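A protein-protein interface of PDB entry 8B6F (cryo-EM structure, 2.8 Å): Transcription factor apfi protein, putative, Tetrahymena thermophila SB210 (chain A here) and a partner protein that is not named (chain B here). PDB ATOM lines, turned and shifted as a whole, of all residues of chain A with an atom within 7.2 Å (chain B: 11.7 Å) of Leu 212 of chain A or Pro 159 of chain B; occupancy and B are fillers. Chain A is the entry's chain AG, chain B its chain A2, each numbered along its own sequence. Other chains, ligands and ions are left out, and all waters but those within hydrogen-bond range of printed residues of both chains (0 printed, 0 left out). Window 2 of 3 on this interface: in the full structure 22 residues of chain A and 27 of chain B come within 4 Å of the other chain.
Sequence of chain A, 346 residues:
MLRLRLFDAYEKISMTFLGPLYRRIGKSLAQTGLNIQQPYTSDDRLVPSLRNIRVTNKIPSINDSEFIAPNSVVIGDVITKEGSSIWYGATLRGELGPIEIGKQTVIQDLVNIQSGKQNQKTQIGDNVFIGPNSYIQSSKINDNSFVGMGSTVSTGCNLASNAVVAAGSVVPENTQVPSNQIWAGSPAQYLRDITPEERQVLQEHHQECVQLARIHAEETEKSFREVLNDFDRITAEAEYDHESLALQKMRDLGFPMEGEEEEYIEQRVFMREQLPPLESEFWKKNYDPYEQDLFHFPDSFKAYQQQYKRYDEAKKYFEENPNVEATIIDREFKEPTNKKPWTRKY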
ATOM      1  N   PHE A  67     -18.673  23.152   8.877  1.00  0.00           N
ATOM      2  CA  PHE A  67     -17.362  23.186   8.244  1.00  0.00           C
ATOM      3  C   PHE A  67     -17.513  23.138   6.734  1.00  0.00           C
ATOM      4  O   PHE A  67     -18.162  22.236   6.200  1.00  0.00           O
ATOM      5  CB  PHE A  67     -16.492  22.017   8.722  1.00  0.00           C
ATOM      6  CG  PHE A  67     -15.170  21.919   8.017  1.00  0.00           C
ATOM      7  CD1 PHE A  67     -14.263  22.960   8.069  1.00  0.00           C
ATOM      8  CD2 PHE A  67     -14.829  20.775   7.316  1.00  0.00           C
ATOM      9  CE1 PHE A  67     -13.045  22.869   7.428  1.00  0.00           C
ATOM     10  CE2 PHE A  67     -13.612  20.677   6.673  1.00  0.00           C
ATOM     11  CZ  PHE A  67     -12.720  21.727   6.728  1.00  0.00           C
ATOM     12  N   SER A  85     -21.198  19.108   6.911  1.00  0.00           N
ATOM     13  CA  SER A  85     -19.777  19.349   6.697  1.00  0.00           C
ATOM     14  C   SER A  85     -19.387  18.974   5.276  1.00  0.00           C
ATOM     15  O   SER A  85     -19.771  17.908   4.784  1.00  0.00           O
ATOM     16  CB  SER A  85     -18.936  18.547   7.692  1.00  0.00           C
ATOM     17  OG  SER A  85     -19.326  18.826   9.025  1.00  0.00           O
ATOM     18  N   TRP A  87     -15.803  18.772   3.064  1.00  0.00           N
ATOM     19  CA  TRP A  87     -14.381  18.731   3.349  1.00  0.00           C
ATOM     20  C   TRP A  87     -13.562  19.097   2.110  1.00  0.00           C
ATOM     21  O   TRP A  87     -14.097  19.487   1.070  1.00  0.00           O
ATOM     22  CB  TRP A  87     -14.021  17.353   3.899  1.00  0.00           C
ATOM     23  CG  TRP A  87     -14.608  17.092   5.253  1.00  0.00           C
ATOM     24  CD1 TRP A  87     -15.928  17.124   5.595  1.00  0.00           C
ATOM     25  CD2 TRP A  87     -13.893  16.760   6.447  1.00  0.00           C
ATOM     26  NE1 TRP A  87     -16.078  16.831   6.925  1.00  0.00           N
ATOM     27  CE2 TRP A  87     -14.844  16.605   7.473  1.00  0.00           C
ATOM     28  CE3 TRP A  87     -12.539  16.579   6.747  1.00  0.00           C
ATOM     29  CZ2 TRP A  87     -14.487  16.276   8.777  1.00  0.00           C
ATOM     30  CZ3 TRP A  87     -12.186  16.253   8.043  1.00  0.00           C
ATOM     31  CH2 TRP A  87     -13.158  16.105   9.043  1.00  0.00           C
ATOM     32  N   GLN A 108     -16.798  13.926   2.738  1.00  0.00           N
ATOM     33  CA  GLN A 108     -15.366  13.948   2.984  1.00  0.00           C
ATOM     34  C   GLN A 108     -14.621  14.463   1.752  1.00  0.00           C
ATOM     35  O   GLN A 108     -15.215  14.992   0.809  1.00  0.00           O
ATOM     36  CB  GLN A 108     -14.899  12.559   3.409  1.00  0.00           C
ATOM     37  CG  GLN A 108     -15.400  12.138   4.778  1.00  0.00           C
ATOM     38  CD  GLN A 108     -14.715  12.886   5.901  1.00  0.00           C
ATOM     39  OE1 GLN A 108     -13.697  13.541   5.695  1.00  0.00           O
ATOM     40  NE2 GLN A 108     -15.273  12.789   7.101  1.00  0.00           N
ATOM     41  N   HIS A 206     -19.299   8.144  12.468  1.00  0.00           N
ATOM     42  CA  HIS A 206     -19.972   9.340  11.975  1.00  0.00           C
ATOM     43  C   HIS A 206     -19.905  10.467  12.996  1.00  0.00           C
ATOM     44  O   HIS A 206     -19.622  11.617  12.645  1.00  0.00           O
ATOM     45  CB  HIS A 206     -21.427   9.027  11.631  1.00  0.00           C
ATOM     46  CG  HIS A 206     -22.223  10.232  11.241  1.00  0.00           C
ATOM     47  ND1 HIS A 206     -22.044  10.887  10.043  1.00  0.00           N
ATOM     48  CD2 HIS A 206     -23.194  10.909  11.898  1.00  0.00           C
ATOM     49  CE1 HIS A 206     -22.874  11.913   9.976  1.00  0.00           C
ATOM     50  NE2 HIS A 206     -23.582  11.949  11.089  1.00  0.00           N
ATOM     51  N   GLN A 207     -20.157  10.154  14.267  1.00  0.00           N
ATOM     52  CA  GLN A 207     -20.085  11.173  15.308  1.00  0.00           C
ATOM     53  C   GLN A 207     -18.670  11.715  15.445  1.00  0.00           C
ATOM     54  O   GLN A 207     -18.474  12.918  15.639  1.00  0.00           O
ATOM     55  CB  GLN A 207     -20.573  10.605  16.640  1.00  0.00           C
ATOM     56  CG  GLN A 207     -22.046  10.235  16.642  1.00  0.00           C
ATOM     57  CD  GLN A 207     -22.476   9.573  17.934  1.00  0.00           C
ATOM     58  OE1 GLN A 207     -21.705   9.482  18.887  1.00  0.00           O
ATOM     59  NE2 GLN A 207     -23.718   9.102  17.970  1.00  0.00           N
ATOM     60  N   GLU A 208     -17.668  10.841  15.345  1.00  0.00           N
ATOM     61  CA  GLU A 208     -16.286  11.297  15.433  1.00  0.00           C
ATOM     62  C   GLU A 208     -15.963  12.271  14.309  1.00  0.00           C
ATOM     63  O   GLU A 208     -15.322  13.303  14.536  1.00  0.00           O
ATOM     64  CB  GLU A 208     -15.341  10.097  15.385  1.00  0.00           C
ATOM     65  CG  GLU A 208     -13.923  10.396  15.841  1.00  0.00           C
ATOM     66  CD  GLU A 208     -13.809  10.515  17.347  1.00  0.00           C
ATOM     67  OE1 GLU A 208     -14.857  10.612  18.019  1.00  0.00           O
ATOM     68  OE2 GLU A 208     -12.672  10.504  17.859  1.00  0.00           O
ATOM     69  N   CYS A 209     -16.400  11.963  13.088  1.00  0.00           N
ATOM     70  CA  CYS A 209     -16.155  12.868  11.971  1.00  0.00           C
ATOM     71  C   CYS A 209     -16.909  14.181  12.145  1.00  0.00           C
ATOM     72  O   CYS A 209     -16.391  15.248  11.803  1.00  0.00           O
ATOM     73  CB  CYS A 209     -16.541  12.189  10.659  1.00  0.00           C
ATOM     74  SG  CYS A 209     -15.525  10.740  10.291  1.00  0.00           S
ATOM     75  N   VAL A 210     -18.139  14.124  12.663  1.00  0.00           N
ATOM     76  CA  VAL A 210     -18.894  15.350  12.908  1.00  0.00           C
ATOM     77  C   VAL A 210     -18.152  16.240  13.897  1.00  0.00           C
ATOM     78  O   VAL A 210     -18.028  17.453  13.697  1.00  0.00           O
ATOM     79  CB  VAL A 210     -20.312  15.012  13.407  1.00  0.00           C
ATOM     80  CG1 VAL A 210     -21.000  16.247  13.978  1.00  0.00           C
ATOM     81  CG2 VAL A 210     -21.143  14.426  12.281  1.00  0.00           C
ATOM     82  N   GLN A 211     -17.648  15.648  14.981  1.00  0.00           N
ATOM     83  CA  GLN A 211     -16.913  16.426  15.973  1.00  0.00           C
ATOM     84  C   GLN A 211     -15.610  16.959  15.396  1.00  0.00           C
ATOM     85  O   GLN A 211     -15.209  18.090  15.691  1.00  0.00           O
ATOM     86  CB  GLN A 211     -16.639  15.576  17.211  1.00  0.00           C
ATOM     87  CG  GLN A 211     -17.889  15.094  17.925  1.00  0.00           C
ATOM     88  CD  GLN A 211     -18.718  16.230  18.484  1.00  0.00           C
ATOM     89  OE1 GLN A 211     -18.281  17.379  18.518  1.00  0.00           O
ATOM     90  NE2 GLN A 211     -19.931  15.912  18.923  1.00  0.00           N
ATOM     91  N   LEU A 212     -14.929  16.150  14.583  1.00  0.00           N
ATOM     92  CA  LEU A 212     -13.670  16.580  13.990  1.00  0.00           C
ATOM     93  C   LEU A 212     -13.871  17.719  13.001  1.00  0.00           C
ATOM     94  O   LEU A 212     -12.964  18.534  12.802  1.00  0.00           O
ATOM     95  CB  LEU A 212     -12.998  15.392  13.306  1.00  0.00           C
ATOM     96  CG  LEU A 212     -11.558  15.571  12.833  1.00  0.00           C
ATOM     97  CD1 LEU A 212     -10.600  15.763  13.999  1.00  0.00           C
ATOM     98  CD2 LEU A 212     -11.165  14.366  12.006  1.00  0.00           C
ATOM     99  N   ALA A 213     -15.043  17.789  12.368  1.00  0.00           N
ATOM    100  CA  ALA A 213     -15.325  18.891  11.456  1.00  0.00           C
ATOM    101  C   ALA A 213     -15.268  20.232  12.177  1.00  0.00           C
ATOM    102  O   ALA A 213     -14.839  21.238  11.602  1.00  0.00           O
ATOM    103  CB  ALA A 213     -16.689  18.691  10.800  1.00  0.00           C
ATOM    104  N   ARG A 214     -15.696  20.266  13.440  1.00  0.00           N
ATOM    105  CA  ARG A 214     -15.622  21.504  14.209  1.00  0.00           C
ATOM    106  C   ARG A 214     -14.180  21.957  14.383  1.00  0.00           C
ATOM    107  O   ARG A 214     -13.872  23.144  14.225  1.00  0.00           O
ATOM    108  CB  ARG A 214     -16.285  21.318  15.573  1.00  0.00           C
ATOM    109  CG  ARG A 214     -17.778  21.073  15.511  1.00  0.00           C
ATOM    110  CD  ARG A 214     -18.381  21.012  16.904  1.00  0.00           C
ATOM    111  NE  ARG A 214     -19.833  20.886  16.860  1.00  0.00           N
ATOM    112  CZ  ARG A 214     -20.490  19.735  16.813  1.00  0.00           C
ATOM    113  NH1 ARG A 214     -19.856  18.575  16.805  1.00  0.00           N
ATOM    114  NH2 ARG A 214     -21.819  19.750  16.772  1.00  0.00           N
ATOM    115  N   ILE A 215     -13.285  21.029  14.715  1.00  0.00           N
ATOM    116  CA  ILE A 215     -11.879  21.380  14.880  1.00  0.00           C
ATOM    117  C   ILE A 215     -11.299  21.869  13.559  1.00  0.00           C
ATOM    118  O   ILE A 215     -10.548  22.851  13.518  1.00  0.00           O
ATOM    119  CB  ILE A 215     -11.092  20.178  15.435  1.00  0.00           C
ATOM    120  CG1 ILE A 215     -11.679  19.741  16.780  1.00  0.00           C
ATOM    121  CG2 ILE A 215      -9.619  20.528  15.580  1.00  0.00           C
ATOM    122  CD1 ILE A 215     -11.121  18.439  17.301  1.00  0.00           C
ATOM    123  N   HIS A 216     -11.632  21.190  12.461  1.00  0.00           N
ATOM    124  CA  HIS A 216     -11.142  21.615  11.154  1.00  0.00           C
ATOM    125  C   HIS A 216     -11.634  23.013  10.811  1.00  0.00           C
ATOM    126  O   HIS A 216     -10.871  23.839  10.300  1.00  0.00           O
ATOM    127  CB  HIS A 216     -11.576  20.620  10.080  1.00  0.00           C
ATOM    128  CG  HIS A 216     -10.666  19.441   9.952  1.00  0.00           C
ATOM    129  ND1 HIS A 216      -9.425  19.520   9.360  1.00  0.00           N
ATOM    130  CD2 HIS A 216     -10.823  18.149  10.322  1.00  0.00           C
ATOM    131  CE1 HIS A 216      -8.852  18.331   9.381  1.00  0.00           C
ATOM    132  NE2 HIS A 216      -9.680  17.481   9.960  1.00  0.00           N
ATOM    133  N   ALA A 217     -12.906  23.298  11.088  1.00  0.00           N
ATOM    134  CA  ALA A 217     -13.439  24.629  10.820  1.00  0.00           C
ATOM    135  C   ALA A 217     -12.729  25.680  11.659  1.00  0.00           C
ATOM    136  O   ALA A 217     -12.399  26.763  11.162  1.00  0.00           O
ATOM    137  CB  ALA A 217     -14.942  24.658  11.090  1.00  0.00           C
ATOM    138  N   GLU A 218     -12.492  25.386  12.936  1.00  0.00           N
ATOM    139  CA  GLU A 218     -11.796  26.339  13.790  1.00  0.00           C
ATOM    140  C   GLU A 218     -10.402  26.640  13.252  1.00  0.00           C
ATOM    141  O   GLU A 218      -9.971  27.798  13.240  1.00  0.00           O
ATOM    142  CB  GLU A 218     -11.715  25.794  15.214  1.00  0.00           C
ATOM    143  CG  GLU A 218     -11.005  26.712  16.195  1.00  0.00           C
ATOM    144  CD  GLU A 218     -10.907  26.109  17.580  1.00  0.00           C
ATOM    145  OE1 GLU A 218     -11.410  24.982  17.774  1.00  0.00           O
ATOM    146  OE2 GLU A 218     -10.324  26.757  18.475  1.00  0.00           O
ATOM    147  N   ASN B 147     -10.848   5.833  27.239  1.00  0.00           N
ATOM    148  CA  ASN B 147     -10.377   5.762  25.858  1.00  0.00           C
ATOM    149  C   ASN B 147      -9.218   4.770  25.719  1.00  0.00           C
ATOM    150  O   ASN B 147      -8.128   5.104  25.253  1.00  0.00           O
ATOM    151  CB  ASN B 147      -9.975   7.151  25.354  1.00  0.00           C
ATOM    152  CG  ASN B 147      -9.636   7.159  23.879  1.00  0.00           C
ATOM    153  OD1 ASN B 147     -10.172   6.372  23.102  1.00  0.00           O
ATOM    154  ND2 ASN B 147      -8.737   8.049  23.484  1.00  0.00           N
ATOM    155  N   LYS B 155      -6.286   4.836  22.244  1.00  0.00           N
ATOM    156  CA  LYS B 155      -6.713   4.881  20.855  1.00  0.00           C
ATOM    157  C   LYS B 155      -6.681   6.320  20.364  1.00  0.00           C
ATOM    158  O   LYS B 155      -6.693   7.268  21.151  1.00  0.00           O
ATOM    159  CB  LYS B 155      -8.125   4.300  20.681  1.00  0.00           C
ATOM    160  CG  LYS B 155      -8.273   2.883  21.208  1.00  0.00           C
ATOM    161  CD  LYS B 155      -9.634   2.290  20.870  1.00  0.00           C
ATOM    162  CE  LYS B 155     -10.760   3.022  21.575  1.00  0.00           C
ATOM    163  NZ  LYS B 155     -12.077   2.384  21.306  1.00  0.00           N
ATOM    164  N   GLY B 156      -6.626   6.474  19.046  1.00  0.00           N
ATOM    165  CA  GLY B 156      -6.663   7.785  18.439  1.00  0.00           C
ATOM    166  C   GLY B 156      -8.052   8.392  18.499  1.00  0.00           C
ATOM    167  O   GLY B 156      -9.025   7.783  18.945  1.00  0.00           O
ATOM    168  N   GLY B 157      -8.137   9.637  18.044  1.00  0.00           N
ATOM    169  CA  GLY B 157      -9.414  10.333  18.053  1.00  0.00           C
ATOM    170  C   GLY B 157      -9.241  11.814  17.804  1.00  0.00           C
ATOM    171  O   GLY B 157      -8.286  12.243  17.149  1.00  0.00           O
ATOM    172  N   LEU B 158     -10.178  12.585  18.332  1.00  0.00           N
ATOM    173  CA  LEU B 158     -10.151  14.026  18.135  1.00  0.00           C
ATOM    174  C   LEU B 158      -8.923  14.623  18.814  1.00  0.00           C
ATOM    175  O   LEU B 158      -8.670  14.330  19.987  1.00  0.00           O
ATOM    176  CB  LEU B 158     -11.417  14.657  18.706  1.00  0.00           C
ATOM    177  CG  LEU B 158     -12.737  14.080  18.195  1.00  0.00           C
ATOM    178  CD1 LEU B 158     -13.898  14.674  18.962  1.00  0.00           C
ATOM    179  CD2 LEU B 158     -12.892  14.329  16.706  1.00  0.00           C
ATOM    180  N   PRO B 159      -8.139  15.452  18.123  1.00  0.00           N
ATOM    181  CA  PRO B 159      -7.031  16.133  18.803  1.00  0.00           C
ATOM    182  C   PRO B 159      -7.543  17.003  19.939  1.00  0.00           C
ATOM    183  O   PRO B 159      -8.616  17.602  19.853  1.00  0.00           O
ATOM    184  CB  PRO B 159      -6.391  16.972  17.692  1.00  0.00           C
ATOM    185  CG  PRO B 159      -6.781  16.294  16.430  1.00  0.00           C
ATOM    186  CD  PRO B 159      -8.141  15.720  16.676  1.00  0.00           C
ATOM    187  N   VAL B 160      -6.762  17.067  21.013  1.00  0.00           N
ATOM    188  CA  VAL B 160      -7.109  17.832  22.203  1.00  0.00           C
ATOM    189  C   VAL B 160      -6.164  19.020  22.307  1.00  0.00           C
ATOM    190  O   VAL B 160      -4.953  18.883  22.102  1.00  0.00           O
ATOM    191  CB  VAL B 160      -7.050  16.966  23.476  1.00  0.00           C
ATOM    192  CG1 VAL B 160      -7.398  17.797  24.696  1.00  0.00           C
ATOM    193  CG2 VAL B 160      -7.985  15.776  23.355  1.00  0.00           C
ATOM    194  N   LYS B 161      -6.719  20.183  22.625  1.00  0.00           N
ATOM    195  CA  LYS B 161      -5.936  21.409  22.676  1.00  0.00           C
ATOM    196  C   LYS B 161      -5.034  21.402  23.903  1.00  0.00           C
ATOM    197  O   LYS B 161      -5.512  21.285  25.036  1.00  0.00           O
ATOM    198  CB  LYS B 161      -6.864  22.620  22.700  1.00  0.00           C
ATOM    199  CG  LYS B 161      -6.147  23.958  22.693  1.00  0.00           C
ATOM    200  CD  LYS B 161      -7.143  25.107  22.703  1.00  0.00           C
ATOM    201  CE  LYS B 161      -6.436  26.452  22.688  1.00  0.00           C
ATOM    202  NZ  LYS B 161      -7.400  27.588  22.713  1.00  0.00           N
ATOM    203  N   GLY B 162      -3.728  21.533  23.678  1.00  0.00           N
ATOM    204  CA  GLY B 162      -2.776  21.657  24.762  1.00  0.00           C
ATOM    205  C   GLY B 162      -2.328  20.360  25.393  1.00  0.00           C
ATOM    206  O   GLY B 162      -1.594  20.403  26.387  1.00  0.00           O
ATOM    207  N   LYS B 163      -2.736  19.208  24.858  1.00  0.00           N
ATOM    208  CA  LYS B 163      -2.364  17.913  25.421  1.00  0.00           C
ATOM    209  C   LYS B 163      -1.535  17.076  24.453  1.00  0.00           C
ATOM    210  O   LYS B 163      -1.508  15.848  24.569  1.00  0.00           O
ATOM    211  CB  LYS B 163      -3.608  17.142  25.864  1.00  0.00           C
ATOM    212  CG  LYS B 163      -4.266  17.723  27.106  1.00  0.00           C
ATOM    213  CD  LYS B 163      -5.354  16.810  27.645  1.00  0.00           C
ATOM    214  CE  LYS B 163      -5.858  17.289  28.993  1.00  0.00           C
ATOM    215  NZ  LYS B 163      -6.338  18.696  28.940  1.00  0.00           N
ATOM    216  N   GLY B 164      -0.858  17.712  23.504  1.00  0.00           N
ATOM    217  CA  GLY B 164       0.046  16.978  22.633  1.00  0.00           C
ATOM    218  C   GLY B 164      -0.670  15.903  21.842  1.00  0.00           C
ATOM    219  O   GLY B 164      -1.723  16.137  21.240  1.00  0.00           O
ATOM    220  N   SER B 165      -0.089  14.704  21.831  1.00  0.00           N
ATOM    221  CA  SER B 165      -0.625  13.594  21.054  1.00  0.00           C
ATOM    222  C   SER B 165      -1.859  12.961  21.681  1.00  0.00           C
ATOM    223  O   SER B 165      -2.500  12.129  21.033  1.00  0.00           O
ATOM    224  CB  SER B 165       0.448  12.519  20.865  1.00  0.00           C
ATOM    225  OG  SER B 165       1.552  13.026  20.136  1.00  0.00           O
ATOM    226  N   ILE B 166      -2.200  13.316  22.921  1.00  0.00           N
ATOM    227  CA  ILE B 166      -3.399  12.769  23.539  1.00  0.00           C
ATOM    228  C   ILE B 166      -4.612  13.176  22.719  1.00  0.00           C
ATOM    229  O   ILE B 166      -4.736  14.327  22.283  1.00  0.00           O
ATOM    230  CB  ILE B 166      -3.524  13.249  24.994  1.00  0.00           C
ATOM    231  CG1 ILE B 166      -2.286  12.831  25.795  1.00  0.00           C
ATOM    232  CG2 ILE B 166      -4.793  12.688  25.628  1.00  0.00           C
ATOM    233  CD1 ILE B 166      -2.264  13.341  27.219  1.00  0.00           C
ATOM    234  N   ARG B 167      -5.519  12.225  22.502  1.00  0.00           N
ATOM    235  CA  ARG B 167      -6.678  12.436  21.650  1.00  0.00           C
ATOM    236  C   ARG B 167      -7.928  11.948  22.366  1.00  0.00           C
ATOM    237  O   ARG B 167      -7.868  11.063  23.222  1.00  0.00           O
ATOM    238  CB  ARG B 167      -6.511  11.723  20.304  1.00  0.00           C
ATOM    239  CG  ARG B 167      -5.097  11.830  19.764  1.00  0.00           C
ATOM    240  CD  ARG B 167      -5.045  11.914  18.258  1.00  0.00           C
ATOM    241  NE  ARG B 167      -3.666  12.024  17.799  1.00  0.00           N
ATOM    242  CZ  ARG B 167      -3.307  12.321  16.559  1.00  0.00           C
ATOM    243  NH1 ARG B 167      -4.204  12.562  15.620  1.00  0.00           N
ATOM    244  NH2 ARG B 167      -2.015  12.374  16.253  1.00  0.00           N
ATOM    245  N   LYS B 168      -9.063  12.539  22.006  1.00  0.00           N
ATOM    246  CA  LYS B 168     -10.316  12.322  22.712  1.00  0.00           C
ATOM    247  C   LYS B 168     -11.144  11.258  22.005  1.00  0.00           C
ATOM    248  O   LYS B 168     -11.294  11.292  20.779  1.00  0.00           O
ATOM    249  CB  LYS B 168     -11.113  13.624  22.812  1.00  0.00           C
ATOM    250  CG  LYS B 168     -12.407  13.488  23.595  1.00  0.00           C
ATOM    251  CD  LYS B 168     -13.063  14.838  23.820  1.00  0.00           C
ATOM    252  CE  LYS B 168     -14.338  14.698  24.633  1.00  0.00           C
ATOM    253  NZ  LYS B 168     -14.978  16.021  24.890  1.00  0.00           N
ATOM    254  N   GLY B 169     -11.670  10.313  22.781  1.00  0.00           N
ATOM    255  CA  GLY B 169     -12.544   9.285  22.265  1.00  0.00           C
ATOM    256  C   GLY B 169     -14.004   9.685  22.346  1.00  0.00           C
ATOM    257  O   GLY B 169     -14.358  10.825  22.647  1.00  0.00           O
ATOM    258  N   ILE B 170     -14.869   8.710  22.063  1.00  0.00           N
ATOM    259  CA  ILE B 170     -16.306   8.965  22.083  1.00  0.00           C
ATOM    260  C   ILE B 170     -16.787   9.205  23.510  1.00  0.00           C
ATOM    261  O   ILE B 170     -17.519  10.162  23.783  1.00  0.00           O
ATOM    262  CB  ILE B 170     -17.067   7.804  21.417  1.00  0.00           C
ATOM    263  CG1 ILE B 170     -16.871   7.810  19.895  1.00  0.00           C
ATOM    264  CG2 ILE B 170     -18.558   7.870  21.732  1.00  0.00           C
ATOM    265  CD1 ILE B 170     -15.486   7.394  19.424  1.00  0.00           C
ATOM    266  N   GLY B 172     -14.806   9.656  26.240  1.00  0.00           N
ATOM    267  CA  GLY B 172     -13.873  10.377  27.079  1.00  0.00           C
ATOM    268  C   GLY B 172     -12.547  10.541  26.373  1.00  0.00           C
ATOM    269  O   GLY B 172     -12.331  10.029  25.271  1.00  0.00           O
ATOM    270  N   GLU B 173     -11.658  11.272  27.034  1.00  0.00           N
ATOM    271  CA  GLU B 173     -10.329  11.550  26.508  1.00  0.00           C
ATOM    272  C   GLU B 173      -9.297  10.684  27.214  1.00  0.00           C
ATOM    273  O   GLU B 173      -9.347  10.507  28.435  1.00  0.00           O
ATOM    274  CB  GLU B 173      -9.970  13.029  26.666  1.00  0.00           C
ATOM    275  CG  GLU B 173     -10.013  13.534  28.098  1.00  0.00           C
ATOM    276  CD  GLU B 173      -9.480  14.947  28.230  1.00  0.00           C
ATOM    277  OE1 GLU B 173      -8.877  15.447  27.258  1.00  0.00           O
ATOM    278  OE2 GLU B 173      -9.665  15.558  29.304  1.00  0.00           O
ATOM    279  N   GLY B 174      -8.365  10.147  26.437  1.00  0.00           N
ATOM    280  CA  GLY B 174      -7.340   9.289  26.987  1.00  0.00           C
ATOM    281  C   GLY B 174      -6.338  10.056  27.826  1.00  0.00           C
ATOM    282  O   GLY B 174      -6.248  11.282  27.797  1.00  0.00           O
ATOM    283  N   GLY B 176      -3.020   9.365  27.633  1.00  0.00           N
ATOM    284  CA  GLY B 176      -1.712   9.195  27.030  1.00  0.00           C
ATOM    285  C   GLY B 176      -1.829   9.159  25.524  1.00  0.00           C
ATOM    286  O   GLY B 176      -2.922   9.238  24.958  1.00  0.00           O
ATOM    287  N   ALA B 177      -0.676   9.028  24.877  1.00  0.00           N
ATOM    288  CA  ALA B 177      -0.630   9.008  23.428  1.00  0.00           C
ATOM    289  C   ALA B 177      -1.311   7.749  22.895  1.00  0.00           C
ATOM    290  O   ALA B 177      -1.467   6.764  23.619  1.00  0.00           O
ATOM    291  CB  ALA B 177       0.814   9.082  22.945  1.00  0.00           C
ATOM    292  N   PRO B 178      -1.733   7.765  21.626  1.00  0.00           N
ATOM    293  CA  PRO B 178      -2.572   6.674  21.105  1.00  0.00           C
ATOM    294  C   PRO B 178      -2.061   5.268  21.388  1.00  0.00           C
ATOM    295  O   PRO B 178      -2.779   4.471  21.997  1.00  0.00           O
ATOM    296  CB  PRO B 178      -2.599   6.959  19.598  1.00  0.00           C
ATOM    297  CG  PRO B 178      -2.457   8.427  19.506  1.00  0.00           C
ATOM    298  CD  PRO B 178      -1.532   8.824  20.621  1.00  0.00           C
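Glu 208 of chain A touches Gly 157 of chain B (OE2 to CA, 3.3 Å). OE1 of Glu 208 of chain A touches CD1 of Ile 170 of chain B, at 3.6 Å. CB of Gln 211 of chain A touches CD1 of Leu 158 of chain B, 3.4 Å away. Leu 212 of chain A touches Leu 158 of chain B (N to CD2, 3.5 Å). CD of Pro 159 of chain B touches CD1 of Leu 212 of chain A, 3.6 Å away. Pro 159 of chain B touches Ile 215 of chain A.
The side-chain carboxylate (OE2) of Glu 208 of chain A sits at hydrogen-bond distance from the backbone NH (N) of Leu 158 of chain B. OE2 of Glu 208 of chain A lies close to O of Lys 168 of chain B, 3.3 Å away.
OE1 of Gln 211 of chain A lies within hydrogen-bond range of NH1 of Arg 214 of chain A, at 2.6 Å. O of Leu 158 of chain B sits at hydrogen-bond distance from N of Lys 168 of chain B, at 2.7 Å.
Printed residues of chain B that touch a printed residue of chain A: Gly 157, Leu 158, Pro 159, Lys 168 and Ile 170. Hydrophobic or aromatic side chains of chain B that line the printed part of chain A: Leu 158, Pro 159 and Ile 170. Printed residues of chain A that touch a printed residue of chain B: Glu 208, Gln 211, Leu 212 and Ile 215. Hydrophobic or aromatic side chains of chain A that line the printed part of chain B: Leu 212 and Ile 215. Among the printed residues, no Asp or Glu carboxylate lies within 4 Å of a Lys or Arg side-chain nitrogen of the other chain.
Leu 212 of chain A touches just these residues of chain B: Leu 158 (3.5 Å) and Pro 159 (3.6 Å). Of chain A, only Leu 212 (3.6 Å) and Ile 215 (3.7 Å) come within 4 Å of Pro 159 of chain B. Of chain B, only Gly 157 (3.3 Å), Leu 158 (3.3 Å), Lys 168 (3.3 Å) and Ile 170 (3.6 Å) come within 4 Å of Glu 208 of chain A. No residue of chain B comes within 4 Å of Cys 209 of chain A. No residue of chain B comes within 4 Å of Val 210 of chain A. Of chain B, only Leu 158 comes within 4 Å of Gln 211 of chain A. No residue of chain B comes within 4 Å of Ala 213 of chain A. Ile 215 of chain A touches just one residue of chain B: Pro 159 (3.7 Å). Of the printed residues of chain A, Ile 170 of chain B touches Glu 208 (3.6 Å). Of the printed residues of chain A, Leu 158 of chain B touches Glu 208 (3.3 Å), Gln 211 (3.4 Å) and Leu 212 (3.5 Å). Printed residues of chain A within 4 Å of Lys 168 of chain B: Glu 208. Gln 207 of chain A touches none of the printed residues of chain B. Gly 174 of chain B touches none of the printed residues of chain A. The nearest residue of chain B that does not touch Leu 212 of chain A is Gly 157 of chain B (5.3 Å). The nearest residue of chain A that does not touch Pro 159 of chain B is Glu 208 of chain A (6.7 Å). The nearest printed residue of chain A that does not touch Ile 170 of chain B is Gln 207 of chain A (4.5 Å).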
